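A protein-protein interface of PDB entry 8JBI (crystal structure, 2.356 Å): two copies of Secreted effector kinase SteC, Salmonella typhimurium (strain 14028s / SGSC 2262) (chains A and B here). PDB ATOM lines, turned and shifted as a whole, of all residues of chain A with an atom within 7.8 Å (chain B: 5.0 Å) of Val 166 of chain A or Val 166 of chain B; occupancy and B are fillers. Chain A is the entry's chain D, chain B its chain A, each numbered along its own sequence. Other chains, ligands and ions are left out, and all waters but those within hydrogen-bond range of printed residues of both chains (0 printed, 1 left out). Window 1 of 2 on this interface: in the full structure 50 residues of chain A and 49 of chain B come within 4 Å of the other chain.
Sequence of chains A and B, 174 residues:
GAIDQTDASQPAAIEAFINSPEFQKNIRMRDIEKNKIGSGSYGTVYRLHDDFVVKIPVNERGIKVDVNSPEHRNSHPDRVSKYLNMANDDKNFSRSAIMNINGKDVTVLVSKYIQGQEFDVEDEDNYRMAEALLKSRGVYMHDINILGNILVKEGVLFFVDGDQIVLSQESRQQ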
ATOM      1  N   TYR A 127      16.864 -20.660  16.684  1.00  0.00           N
ATOM      2  CA  TYR A 127      16.487 -20.304  15.327  1.00  0.00           C
ATOM      3  C   TYR A 127      17.731 -20.331  14.463  1.00  0.00           C
ATOM      4  O   TYR A 127      17.735 -20.922  13.389  1.00  0.00           O
ATOM      5  CB  TYR A 127      15.816 -18.910  15.292  1.00  0.00           C
ATOM      6  CG  TYR A 127      15.475 -18.412  13.891  1.00  0.00           C
ATOM      7  CD1 TYR A 127      16.453 -17.853  13.063  1.00  0.00           C
ATOM      8  CD2 TYR A 127      14.178 -18.508  13.392  1.00  0.00           C
ATOM      9  CE1 TYR A 127      16.144 -17.406  11.786  1.00  0.00           C
ATOM     10  CE2 TYR A 127      13.861 -18.059  12.109  1.00  0.00           C
ATOM     11  CZ  TYR A 127      14.848 -17.510  11.318  1.00  0.00           C
ATOM     12  OH  TYR A 127      14.557 -17.059  10.051  1.00  0.00           O
ATOM     13  N   LEU A 134      19.742 -26.254   8.118  1.00  0.00           N
ATOM     14  CA  LEU A 134      19.013 -26.299   6.853  1.00  0.00           C
ATOM     15  C   LEU A 134      19.822 -25.756   5.700  1.00  0.00           C
ATOM     16  O   LEU A 134      19.755 -26.268   4.589  1.00  0.00           O
ATOM     17  CB  LEU A 134      17.702 -25.536   6.970  1.00  0.00           C
ATOM     18  CG  LEU A 134      16.673 -26.302   7.787  1.00  0.00           C
ATOM     19  CD1 LEU A 134      15.481 -25.426   8.135  1.00  0.00           C
ATOM     20  CD2 LEU A 134      16.245 -27.532   7.016  1.00  0.00           C
ATOM     21  N   VAL A 139      18.670 -25.649   2.060  1.00  0.00           N
ATOM     22  CA  VAL A 139      17.316 -25.235   2.393  1.00  0.00           C
ATOM     23  C   VAL A 139      17.312 -23.888   3.084  1.00  0.00           C
ATOM     24  O   VAL A 139      18.040 -23.681   4.079  1.00  0.00           O
ATOM     25  CB  VAL A 139      16.611 -26.253   3.302  1.00  0.00           C
ATOM     26  CG1 VAL A 139      15.280 -25.697   3.789  1.00  0.00           C
ATOM     27  CG2 VAL A 139      16.398 -27.567   2.583  1.00  0.00           C
ATOM     28  N   TYR A 140      16.498 -22.976   2.547  1.00  0.00           N
ATOM     29  CA  TYR A 140      16.241 -21.671   3.166  1.00  0.00           C
ATOM     30  C   TYR A 140      15.112 -21.768   4.201  1.00  0.00           C
ATOM     31  O   TYR A 140      14.058 -22.364   3.934  1.00  0.00           O
ATOM     32  CB  TYR A 140      15.861 -20.654   2.076  1.00  0.00           C
ATOM     33  CG  TYR A 140      15.324 -19.338   2.599  1.00  0.00           C
ATOM     34  CD1 TYR A 140      16.189 -18.320   2.994  1.00  0.00           C
ATOM     35  CD2 TYR A 140      13.955 -19.118   2.700  1.00  0.00           C
ATOM     36  CE1 TYR A 140      15.705 -17.116   3.481  1.00  0.00           C
ATOM     37  CE2 TYR A 140      13.457 -17.916   3.165  1.00  0.00           C
ATOM     38  CZ  TYR A 140      14.336 -16.920   3.560  1.00  0.00           C
ATOM     39  OH  TYR A 140      13.833 -15.728   4.027  1.00  0.00           O
ATOM     40  N   MET A 141      15.331 -21.174   5.372  1.00  0.00           N
ATOM     41  CA  MET A 141      14.341 -21.181   6.437  1.00  0.00           C
ATOM     42  C   MET A 141      13.915 -19.749   6.800  1.00  0.00           C
ATOM     43  O   MET A 141      14.724 -18.813   6.798  1.00  0.00           O
ATOM     44  CB  MET A 141      14.921 -21.887   7.680  1.00  0.00           C
ATOM     45  CG  MET A 141      14.015 -21.865   8.943  1.00  0.00           C
ATOM     46  SD  MET A 141      14.695 -22.723  10.410  1.00  0.00           S
ATOM     47  CE  MET A 141      14.911 -21.342  11.516  1.00  0.00           C
ATOM     48  N   HIS A 142      12.653 -19.582   7.149  1.00  0.00           N
ATOM     49  CA  HIS A 142      12.203 -18.280   7.634  1.00  0.00           C
ATOM     50  C   HIS A 142      11.034 -18.437   8.584  1.00  0.00           C
ATOM     51  O   HIS A 142      10.258 -19.384   8.488  1.00  0.00           O
ATOM     52  CB  HIS A 142      11.791 -17.355   6.463  1.00  0.00           C
ATOM     53  CG  HIS A 142      11.867 -15.898   6.793  1.00  0.00           C
ATOM     54  ND1 HIS A 142      10.780 -15.180   7.251  1.00  0.00           N
ATOM     55  CD2 HIS A 142      12.904 -15.027   6.747  1.00  0.00           C
ATOM     56  CE1 HIS A 142      11.145 -13.924   7.465  1.00  0.00           C
ATOM     57  NE2 HIS A 142      12.427 -13.806   7.163  1.00  0.00           N
ATOM     58  N   ASP A 143      10.906 -17.489   9.497  1.00  0.00           N
ATOM     59  CA  ASP A 143       9.679 -17.345  10.251  1.00  0.00           C
ATOM     60  C   ASP A 143       8.534 -17.121   9.266  1.00  0.00           C
ATOM     61  O   ASP A 143       8.756 -16.803   8.081  1.00  0.00           O
ATOM     62  CB  ASP A 143       9.794 -16.150  11.188  1.00  0.00           C
ATOM     63  CG  ASP A 143       8.615 -16.037  12.130  1.00  0.00           C
ATOM     64  OD1 ASP A 143       7.987 -17.077  12.454  1.00  0.00           O
ATOM     65  OD2 ASP A 143       8.323 -14.897  12.539  1.00  0.00           O
ATOM     66  N   ILE A 144       7.307 -17.287   9.742  1.00  0.00           N
ATOM     67  CA  ILE A 144       6.150 -17.099   8.877  1.00  0.00           C
ATOM     68  C   ILE A 144       5.605 -15.680   8.990  1.00  0.00           C
ATOM     69  O   ILE A 144       4.484 -15.408   8.575  1.00  0.00           O
ATOM     70  CB  ILE A 144       5.029 -18.074   9.231  1.00  0.00           C
ATOM     71  CG1 ILE A 144       4.708 -17.974  10.714  1.00  0.00           C
ATOM     72  CG2 ILE A 144       5.412 -19.512   8.865  1.00  0.00           C
ATOM     73  CD1 ILE A 144       3.487 -18.737  11.078  1.00  0.00           C
ATOM     74  N   ASN A 145       6.435 -14.788   9.528  1.00  0.00           N
ATOM     75  CA  ASN A 145       6.024 -13.365   9.586  1.00  0.00           C
ATOM     76  C   ASN A 145       6.540 -12.669   8.323  1.00  0.00           C
ATOM     77  O   ASN A 145       7.498 -13.185   7.713  1.00  0.00           O
ATOM     78  CB  ASN A 145       6.469 -12.692  10.886  1.00  0.00           C
ATOM     79  CG  ASN A 145       5.462 -12.882  12.000  1.00  0.00           C
ATOM     80  OD1 ASN A 145       4.287 -13.136  11.743  1.00  0.00           O
ATOM     81  ND2 ASN A 145       5.911 -12.765  13.239  1.00  0.00           N
ATOM     82  N   ILE A 146       5.919 -11.555   7.949  1.00  0.00           N
ATOM     83  CA  ILE A 146       6.295 -10.788   6.718  1.00  0.00           C
ATOM     84  C   ILE A 146       6.205 -11.636   5.445  1.00  0.00           C
ATOM     85  O   ILE A 146       7.164 -11.625   4.652  1.00  0.00           O
ATOM     86  CB  ILE A 146       7.606 -10.019   6.834  1.00  0.00           C
ATOM     87  CG1 ILE A 146       7.899  -9.580   8.266  1.00  0.00           C
ATOM     88  CG2 ILE A 146       7.373  -8.850   5.933  1.00  0.00           C
ATOM     89  CD1 ILE A 146       6.944  -8.527   8.779  1.00  0.00           C
ATOM     90  N   LEU A 147       5.069 -12.303   5.253  1.00  0.00           N
ATOM     91  CA  LEU A 147       4.788 -13.088   4.025  1.00  0.00           C
ATOM     92  C   LEU A 147       3.806 -12.332   3.115  1.00  0.00           C
ATOM     93  O   LEU A 147       3.029 -11.550   3.624  1.00  0.00           O
ATOM     94  CB  LEU A 147       4.179 -14.431   4.422  1.00  0.00           C
ATOM     95  CG  LEU A 147       5.014 -15.325   5.330  1.00  0.00           C
ATOM     96  CD1 LEU A 147       4.435 -16.727   5.362  1.00  0.00           C
ATOM     97  CD2 LEU A 147       6.462 -15.361   4.881  1.00  0.00           C
ATOM     98  N   GLY A 148       3.821 -12.610   1.812  1.00  0.00           N
ATOM     99  CA  GLY A 148       2.948 -11.896   0.877  1.00  0.00           C
ATOM    100  C   GLY A 148       2.587 -12.600  -0.411  1.00  0.00           C
ATOM    101  O   GLY A 148       3.122 -13.650  -0.666  1.00  0.00           O
ATOM    102  N   ASN A 149       1.684 -12.000  -1.186  1.00  0.00           N
ATOM    103  CA  ASN A 149       1.275 -12.520  -2.510  1.00  0.00           C
ATOM    104  C   ASN A 149       1.574 -11.446  -3.559  1.00  0.00           C
ATOM    105  O   ASN A 149       1.568 -10.290  -3.186  1.00  0.00           O
ATOM    106  CB  ASN A 149      -0.205 -12.872  -2.515  1.00  0.00           C
ATOM    107  CG  ASN A 149      -0.578 -14.007  -1.595  1.00  0.00           C
ATOM    108  OD1 ASN A 149       0.279 -14.762  -1.153  1.00  0.00           O
ATOM    109  ND2 ASN A 149      -1.861 -14.132  -1.308  1.00  0.00           N
ATOM    110  N   GLY A 162      -0.418 -11.968   2.367  1.00  0.00           N
ATOM    111  CA  GLY A 162      -0.717 -13.299   1.848  1.00  0.00           C
ATOM    112  C   GLY A 162       0.291 -14.344   2.284  1.00  0.00           C
ATOM    113  O   GLY A 162       0.858 -14.213   3.364  1.00  0.00           O
ATOM    114  N   ASP A 163       0.542 -15.360   1.452  1.00  0.00           N
ATOM    115  CA  ASP A 163       1.451 -16.452   1.848  1.00  0.00           C
ATOM    116  C   ASP A 163       2.208 -17.154   0.701  1.00  0.00           C
ATOM    117  O   ASP A 163       2.493 -18.344   0.788  1.00  0.00           O
ATOM    118  CB  ASP A 163       0.691 -17.502   2.659  1.00  0.00           C
ATOM    119  CG  ASP A 163      -0.541 -18.015   1.937  1.00  0.00           C
ATOM    120  OD1 ASP A 163      -0.647 -17.816   0.704  1.00  0.00           O
ATOM    121  OD2 ASP A 163      -1.407 -18.616   2.609  1.00  0.00           O
ATOM    122  N   GLN A 164       2.546 -16.410  -0.348  1.00  0.00           N
ATOM    123  CA  GLN A 164       3.228 -16.942  -1.523  1.00  0.00           C
ATOM    124  C   GLN A 164       4.729 -16.742  -1.388  1.00  0.00           C
ATOM    125  O   GLN A 164       5.532 -17.589  -1.810  1.00  0.00           O
ATOM    126  CB  GLN A 164       2.699 -16.218  -2.768  1.00  0.00           C
ATOM    127  CG  GLN A 164       3.330 -16.556  -4.103  1.00  0.00           C
ATOM    128  CD  GLN A 164       2.791 -15.640  -5.222  1.00  0.00           C
ATOM    129  OE1 GLN A 164       2.149 -14.622  -4.940  1.00  0.00           O
ATOM    130  NE2 GLN A 164       3.039 -16.008  -6.484  1.00  0.00           N
ATOM    131  N   ILE A 165       5.118 -15.622  -0.781  1.00  0.00           N
ATOM    132  CA  ILE A 165       6.534 -15.279  -0.708  1.00  0.00           C
ATOM    133  C   ILE A 165       6.882 -14.673   0.624  1.00  0.00           C
ATOM    134  O   ILE A 165       6.011 -14.249   1.364  1.00  0.00           O
ATOM    135  CB  ILE A 165       6.974 -14.282  -1.815  1.00  0.00           C
ATOM    136  CG1 ILE A 165       6.091 -13.039  -1.794  1.00  0.00           C
ATOM    137  CG2 ILE A 165       6.922 -14.934  -3.197  1.00  0.00           C
ATOM    138  CD1 ILE A 165       6.704 -11.856  -2.468  1.00  0.00           C
ATOM    139  N   VAL A 166       8.178 -14.634   0.907  1.00  0.00           N
ATOM    140  CA  VAL A 166       8.699 -14.010   2.106  1.00  0.00           C
ATOM    141  C   VAL A 166       9.151 -12.609   1.750  1.00  0.00           C
ATOM    142  O   VAL A 166       9.836 -12.420   0.750  1.00  0.00           O
ATOM    143  CB  VAL A 166       9.936 -14.784   2.638  1.00  0.00           C
ATOM    144  CG1 VAL A 166      10.752 -13.902   3.562  1.00  0.00           C
ATOM    145  CG2 VAL A 166       9.513 -16.082   3.320  1.00  0.00           C
ATOM    146  N   LEU A 167       8.783 -11.633   2.570  1.00  0.00           N
ATOM    147  CA  LEU A 167       9.250 -10.268   2.378  1.00  0.00           C
ATOM    148  C   LEU A 167      10.163  -9.876   3.533  1.00  0.00           C
ATOM    149  O   LEU A 167       9.682  -9.547   4.610  1.00  0.00           O
ATOM    150  CB  LEU A 167       8.053  -9.305   2.323  1.00  0.00           C
ATOM    151  CG  LEU A 167       6.992  -9.509   1.235  1.00  0.00           C
ATOM    152  CD1 LEU A 167       5.788  -8.618   1.475  1.00  0.00           C
ATOM    153  CD2 LEU A 167       7.584  -9.205  -0.105  1.00  0.00           C
ATOM    154  N   SER A 168      11.474  -9.901   3.333  1.00  0.00           N
ATOM    155  CA  SER A 168      12.363  -9.614   4.459  1.00  0.00           C
ATOM    156  C   SER A 168      13.210  -8.398   4.165  1.00  0.00           C
ATOM    157  O   SER A 168      13.279  -7.944   3.024  1.00  0.00           O
ATOM    158  CB  SER A 168      13.259 -10.813   4.781  1.00  0.00           C
ATOM    159  OG  SER A 168      14.474 -10.733   4.070  1.00  0.00           O
ATOM    160  N   GLN A 169      13.845  -7.858   5.195  1.00  0.00           N
ATOM    161  CA  GLN A 169      14.745  -6.727   4.999  1.00  0.00           C
ATOM    162  C   GLN A 169      16.194  -7.183   5.075  1.00  0.00           C
ATOM    163  O   GLN A 169      17.108  -6.366   4.944  1.00  0.00           O
ATOM    164  CB  GLN A 169      14.496  -5.643   6.035  1.00  0.00           C
ATOM    165  CG  GLN A 169      13.151  -4.967   5.915  1.00  0.00           C
ATOM    166  CD  GLN A 169      13.119  -3.636   6.652  1.00  0.00           C
ATOM    167  OE1 GLN A 169      13.648  -2.635   6.167  1.00  0.00           O
ATOM    168  NE2 GLN A 169      12.512  -3.624   7.837  1.00  0.00           N
ATOM    169  N   TYR B 140      13.898  -8.156   0.273  1.00  0.00           N
ATOM    170  CA  TYR B 140      14.518  -9.342  -0.286  1.00  0.00           C
ATOM    171  C   TYR B 140      13.458 -10.422  -0.344  1.00  0.00           C
ATOM    172  O   TYR B 140      12.771 -10.699   0.631  1.00  0.00           O
ATOM    173  CB  TYR B 140      15.787  -9.708   0.517  1.00  0.00           C
ATOM    174  CG  TYR B 140      16.699  -8.495   0.597  1.00  0.00           C
ATOM    175  CD1 TYR B 140      16.523  -7.520   1.594  1.00  0.00           C
ATOM    176  CD2 TYR B 140      17.675  -8.274  -0.369  1.00  0.00           C
ATOM    177  CE1 TYR B 140      17.323  -6.388   1.641  1.00  0.00           C
ATOM    178  CE2 TYR B 140      18.477  -7.145  -0.333  1.00  0.00           C
ATOM    179  CZ  TYR B 140      18.296  -6.209   0.669  1.00  0.00           C
ATOM    180  OH  TYR B 140      19.097  -5.094   0.700  1.00  0.00           O
ATOM    181  N   MET B 141      13.267 -10.978  -1.523  1.00  0.00           N
ATOM    182  CA  MET B 141      12.140 -11.858  -1.744  1.00  0.00           C
ATOM    183  C   MET B 141      12.637 -13.290  -1.625  1.00  0.00           C
ATOM    184  O   MET B 141      13.789 -13.582  -1.912  1.00  0.00           O
ATOM    185  CB  MET B 141      11.570 -11.599  -3.143  1.00  0.00           C
ATOM    186  CG  MET B 141      10.316 -12.360  -3.494  1.00  0.00           C
ATOM    187  SD  MET B 141       9.875 -12.108  -5.223  1.00  0.00           S
ATOM    188  CE  MET B 141      10.956 -13.328  -5.938  1.00  0.00           C
ATOM    189  N   HIS B 142      11.767 -14.181  -1.189  1.00  0.00           N
ATOM    190  CA  HIS B 142      12.112 -15.584  -1.141  1.00  0.00           C
ATOM    191  C   HIS B 142      10.855 -16.377  -1.410  1.00  0.00           C
ATOM    192  O   HIS B 142       9.798 -16.098  -0.852  1.00  0.00           O
ATOM    193  CB  HIS B 142      12.747 -15.953   0.216  1.00  0.00           C
ATOM    194  CG  HIS B 142      14.181 -15.514   0.352  1.00  0.00           C
ATOM    195  ND1 HIS B 142      14.550 -14.354   1.009  1.00  0.00           N
ATOM    196  CD2 HIS B 142      15.332 -16.068  -0.110  1.00  0.00           C
ATOM    197  CE1 HIS B 142      15.864 -14.215   0.946  1.00  0.00           C
ATOM    198  NE2 HIS B 142      16.362 -15.240   0.274  1.00  0.00           N
ATOM    199  N   ILE B 144       8.329 -19.615  -1.315  1.00  0.00           N
ATOM    200  CA  ILE B 144       7.960 -20.540  -0.255  1.00  0.00           C
ATOM    201  C   ILE B 144       7.583 -21.843  -0.920  1.00  0.00           C
ATOM    202  O   ILE B 144       6.655 -21.875  -1.721  1.00  0.00           O
ATOM    203  CB  ILE B 144       6.748 -20.045   0.546  1.00  0.00           C
ATOM    204  CG1 ILE B 144       7.055 -18.727   1.250  1.00  0.00           C
ATOM    205  CG2 ILE B 144       6.311 -21.085   1.570  1.00  0.00           C
ATOM    206  CD1 ILE B 144       5.838 -18.120   1.935  1.00  0.00           C
ATOM    207  N   ILE B 146       7.224 -25.036   0.993  1.00  0.00           N
ATOM    208  CA  ILE B 146       6.289 -25.627   1.952  1.00  0.00           C
ATOM    209  C   ILE B 146       6.443 -24.987   3.315  1.00  0.00           C
ATOM    210  O   ILE B 146       7.359 -24.199   3.556  1.00  0.00           O
ATOM    211  CB  ILE B 146       6.506 -27.150   2.167  1.00  0.00           C
ATOM    212  CG1 ILE B 146       7.902 -27.426   2.728  1.00  0.00           C
ATOM    213  CG2 ILE B 146       6.254 -27.955   0.897  1.00  0.00           C
ATOM    214  CD1 ILE B 146       8.041 -28.819   3.307  1.00  0.00           C
ATOM    215  N   LEU B 147       5.544 -25.352   4.216  1.00  0.00           N
ATOM    216  CA  LEU B 147       5.641 -24.994   5.622  1.00  0.00           C
ATOM    217  C   LEU B 147       5.878 -26.287   6.397  1.00  0.00           C
ATOM    218  O   LEU B 147       5.428 -27.351   5.968  1.00  0.00           O
ATOM    219  CB  LEU B 147       4.338 -24.347   6.094  1.00  0.00           C
ATOM    220  CG  LEU B 147       4.121 -22.840   5.941  1.00  0.00           C
ATOM    221  CD1 LEU B 147       4.636 -22.325   4.641  1.00  0.00           C
ATOM    222  CD2 LEU B 147       2.651 -22.531   6.081  1.00  0.00           C
ATOM    223  N   GLN B 164       4.802 -23.794  11.067  1.00  0.00           N
ATOM    224  CA  GLN B 164       5.454 -22.828  11.945  1.00  0.00           C
ATOM    225  C   GLN B 164       6.637 -22.096  11.310  1.00  0.00           C
ATOM    226  O   GLN B 164       7.033 -21.011  11.763  1.00  0.00           O
ATOM    227  CB  GLN B 164       5.866 -23.482  13.262  1.00  0.00           C
ATOM    228  CG  GLN B 164       4.688 -24.034  14.084  1.00  0.00           C
ATOM    229  CD  GLN B 164       3.740 -22.956  14.634  1.00  0.00           C
ATOM    230  OE1 GLN B 164       3.846 -21.768  14.306  1.00  0.00           O
ATOM    231  NE2 GLN B 164       2.804 -23.380  15.482  1.00  0.00           N
ATOM    232  N   ILE B 165       7.213 -22.693  10.271  1.00  0.00           N
ATOM    233  CA  ILE B 165       8.307 -22.042   9.562  1.00  0.00           C
ATOM    234  C   ILE B 165       8.153 -22.275   8.072  1.00  0.00           C
ATOM    235  O   ILE B 165       7.511 -23.245   7.647  1.00  0.00           O
ATOM    236  CB  ILE B 165       9.677 -22.584   9.997  1.00  0.00           C
ATOM    237  CG1 ILE B 165       9.728 -24.097   9.797  1.00  0.00           C
ATOM    238  CG2 ILE B 165       9.972 -22.219  11.448  1.00  0.00           C
ATOM    239  CD1 ILE B 165      11.124 -24.645   9.747  1.00  0.00           C
ATOM    240  N   VAL B 166       8.736 -21.402   7.264  1.00  0.00           N
ATOM    241  CA  VAL B 166       8.780 -21.711   5.842  1.00  0.00           C
ATOM    242  C   VAL B 166      10.042 -22.495   5.523  1.00  0.00           C
ATOM    243  O   VAL B 166      11.101 -22.296   6.141  1.00  0.00           O
ATOM    244  CB  VAL B 166       8.651 -20.460   4.930  1.00  0.00           C
ATOM    245  CG1 VAL B 166       7.595 -19.491   5.482  1.00  0.00           C
ATOM    246  CG2 VAL B 166       9.984 -19.772   4.751  1.00  0.00           C
ATOM    247  N   LEU B 167       9.907 -23.402   4.566  1.00  0.00           N
ATOM    248  CA  LEU B 167      11.020 -24.187   4.086  1.00  0.00           C
ATOM    249  C   LEU B 167      11.015 -24.139   2.572  1.00  0.00           C
ATOM    250  O   LEU B 167      10.109 -24.667   1.927  1.00  0.00           O
ATOM    251  CB  LEU B 167      10.854 -25.634   4.523  1.00  0.00           C
ATOM    252  CG  LEU B 167      10.968 -25.920   6.006  1.00  0.00           C
ATOM    253  CD1 LEU B 167      10.665 -27.385   6.254  1.00  0.00           C
ATOM    254  CD2 LEU B 167      12.368 -25.565   6.453  1.00  0.00           C
ATOM    255  N   SER B 168      12.030 -23.523   1.990  1.00  0.00           N
ATOM    256  CA  SER B 168      12.092 -23.493   0.546  1.00  0.00           C
ATOM    257  C   SER B 168      13.501 -23.786   0.061  1.00  0.00           C
ATOM    258  O   SER B 168      14.480 -23.460   0.732  1.00  0.00           O
ATOM    259  CB  SER B 168      11.583 -22.145   0.014  1.00  0.00           C
ATOM    260  OG  SER B 168      12.575 -21.135   0.118  1.00  0.00           O
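The backbone carbonyl oxygen of Val 166 of chain A lies close to the backbone carbonyl oxygen of Tyr 140 of chain B. ND1 of His 142 of chain B is in hydrogen-bond range of OH of Tyr 140 of chain A (3.4 Å). The backbone NH (N) of Val 166 of chain B lies within hydrogen-bond range of the backbone carbonyl oxygen (O) of His 142 of chain A (2.8 Å). The backbone carbonyl oxygen (O) of Gln 164 of chain A lies within hydrogen-bond range of the backbone NH (N) of Ile 144 of chain B (3.5 Å). The backbone NH of Val 166 of chain A is in hydrogen-bond range of the backbone carbonyl oxygen of His 142 of chain B, 2.8 Å away. O of Ser 168 of chain A lies within hydrogen-bond range of N of Tyr 140 of chain B (2.8 Å). O of Ser 168 of chain B sits at hydrogen-bond distance from N of Tyr 140 of chain A.
OD2 of Asp 143 of chain A sits at hydrogen-bond distance from ND2 of Asn 145 of chain A, at 3.3 Å. OD1 of Asn 149 of chain A is in hydrogen-bond range of N of Asp 163 of chain A. The backbone NH of Gly 148 of chain A is in hydrogen-bond range of the backbone carbonyl oxygen of Ile 165 of chain A (2.8 Å). O of Gly 148 of chain A is in hydrogen-bond range of N of Gln 164 of chain A. OD1 of Asn 149 of chain A is in hydrogen-bond range of N of Gln 164 of chain A (2.9 Å). O of Ile 146 of chain B is in hydrogen-bond range of N of Leu 167 of chain B, 2.9 Å away.
Among the printed residues, merely in contact across the chains: Gln 169 of chain A with Tyr 140 of chain B (3.3 Å), Ile 165 of chain A with His 142 of chain B (3.4 Å), Met 141 of chain A with Val 166 of chain B (3.4 Å), Val 166 of chain A with Met 141 of chain B (3.4 Å), His 142 of chain A with Ile 165 of chain B (3.5 Å), Leu 134 of chain A with Leu 167 of chain B (3.5 Å), Asp 163 of chain A with Ile 144 of chain B (3.5 Å), Tyr 140 of chain A with Leu 167 of chain B (3.5 Å), Ile 144 of chain A with Gln 164 of chain B (3.6 Å), Tyr 140 of chain A with Val 166 of chain B (3.7 Å), Val 139 of chain A with Ser 168 of chain B (3.7 Å), Ile 165 of chain A with Ile 144 of chain B (3.8 Å), Ile 165 of chain A with Met 141 of chain B (3.8 Å), Ile 144 of chain A with Ile 165 of chain B (3.9 Å), Asp 143 of chain A with Val 166 of chain B (3.9 Å), Val 139 of chain A with Leu 167 of chain B (3.9 Å), Leu 167 of chain A with Tyr 140 of chain B (3.95 Å), Leu 147 of chain A with Ile 144 of chain B (3.96 Å) and Val 166 of chain A with Val 166 of chain B (3.99 Å).
Printed residues of chain B within 4 Å of His 142 of chain A: Ile 165 and Val 166. Of the printed residues of chain B, Ile 144 of chain A touches Gln 164 (3.6 Å) and Ile 165 (3.9 Å). Gly 148 of chain A touches none of the printed residues of chain B. Printed residues of chain B within 4 Å of Val 166 of chain A: Tyr 140, Met 141, His 142 and Val 166. Printed residues of chain B within 4 Å of Leu 167 of chain A: Tyr 140 (3.95 Å). Printed residues of chain A within 4 Å of Val 166 of chain B: Tyr 140 (3.7 Å), Met 141 (3.4 Å), His 142 (2.8 Å), Asp 143 (3.9 Å) and Val 166 (3.99 Å). The nearest printed residue of chain A that does not touch Val 166 of chain B is Ile 144 of chain A (4.03 Å).
Of the 21 printed residues of chain A, 15 touch a printed residue of chain B. Hydrophobic or aromatic side chains of chain A within 4 Å of the printed part of chain B: Leu 134, Val 139, Tyr 140, His 142, Ile 144, Leu 147, Ile 165 and Val 166. Of the 11 printed residues of chain B, 9 touch a printed residue of chain A. Among the printed residues, 26 pairs touch across the chains. Among the printed residues, no Asp or Glu carboxylate lies within 4 Å of a Lys or Arg side-chain nitrogen of the other chain.
Tyr 140 of chain A touches Ser 168 of chain B, and with the chains exchanged Ser 168 of chain A touches Tyr 140 of chain B. His 142 of chain A touches Ile 165 of chain B, and with the chains exchanged Ile 165 of chain A touches His 142 of chain B. Ile 144 of chain A touches Gln 164 of chain B, and with the chains exchanged Gln 164 of chain A touches Ile 144 of chain B. Ile 165 of chain A touches Met 141 of chain B, but with the chains exchanged Met 141 of chain A does not touch Ile 165 of chain B (4.1 Å). Positions printed for both chains: 140, 141, 142, 144, 146, 147, 164, 165, 166, 167 and 168.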
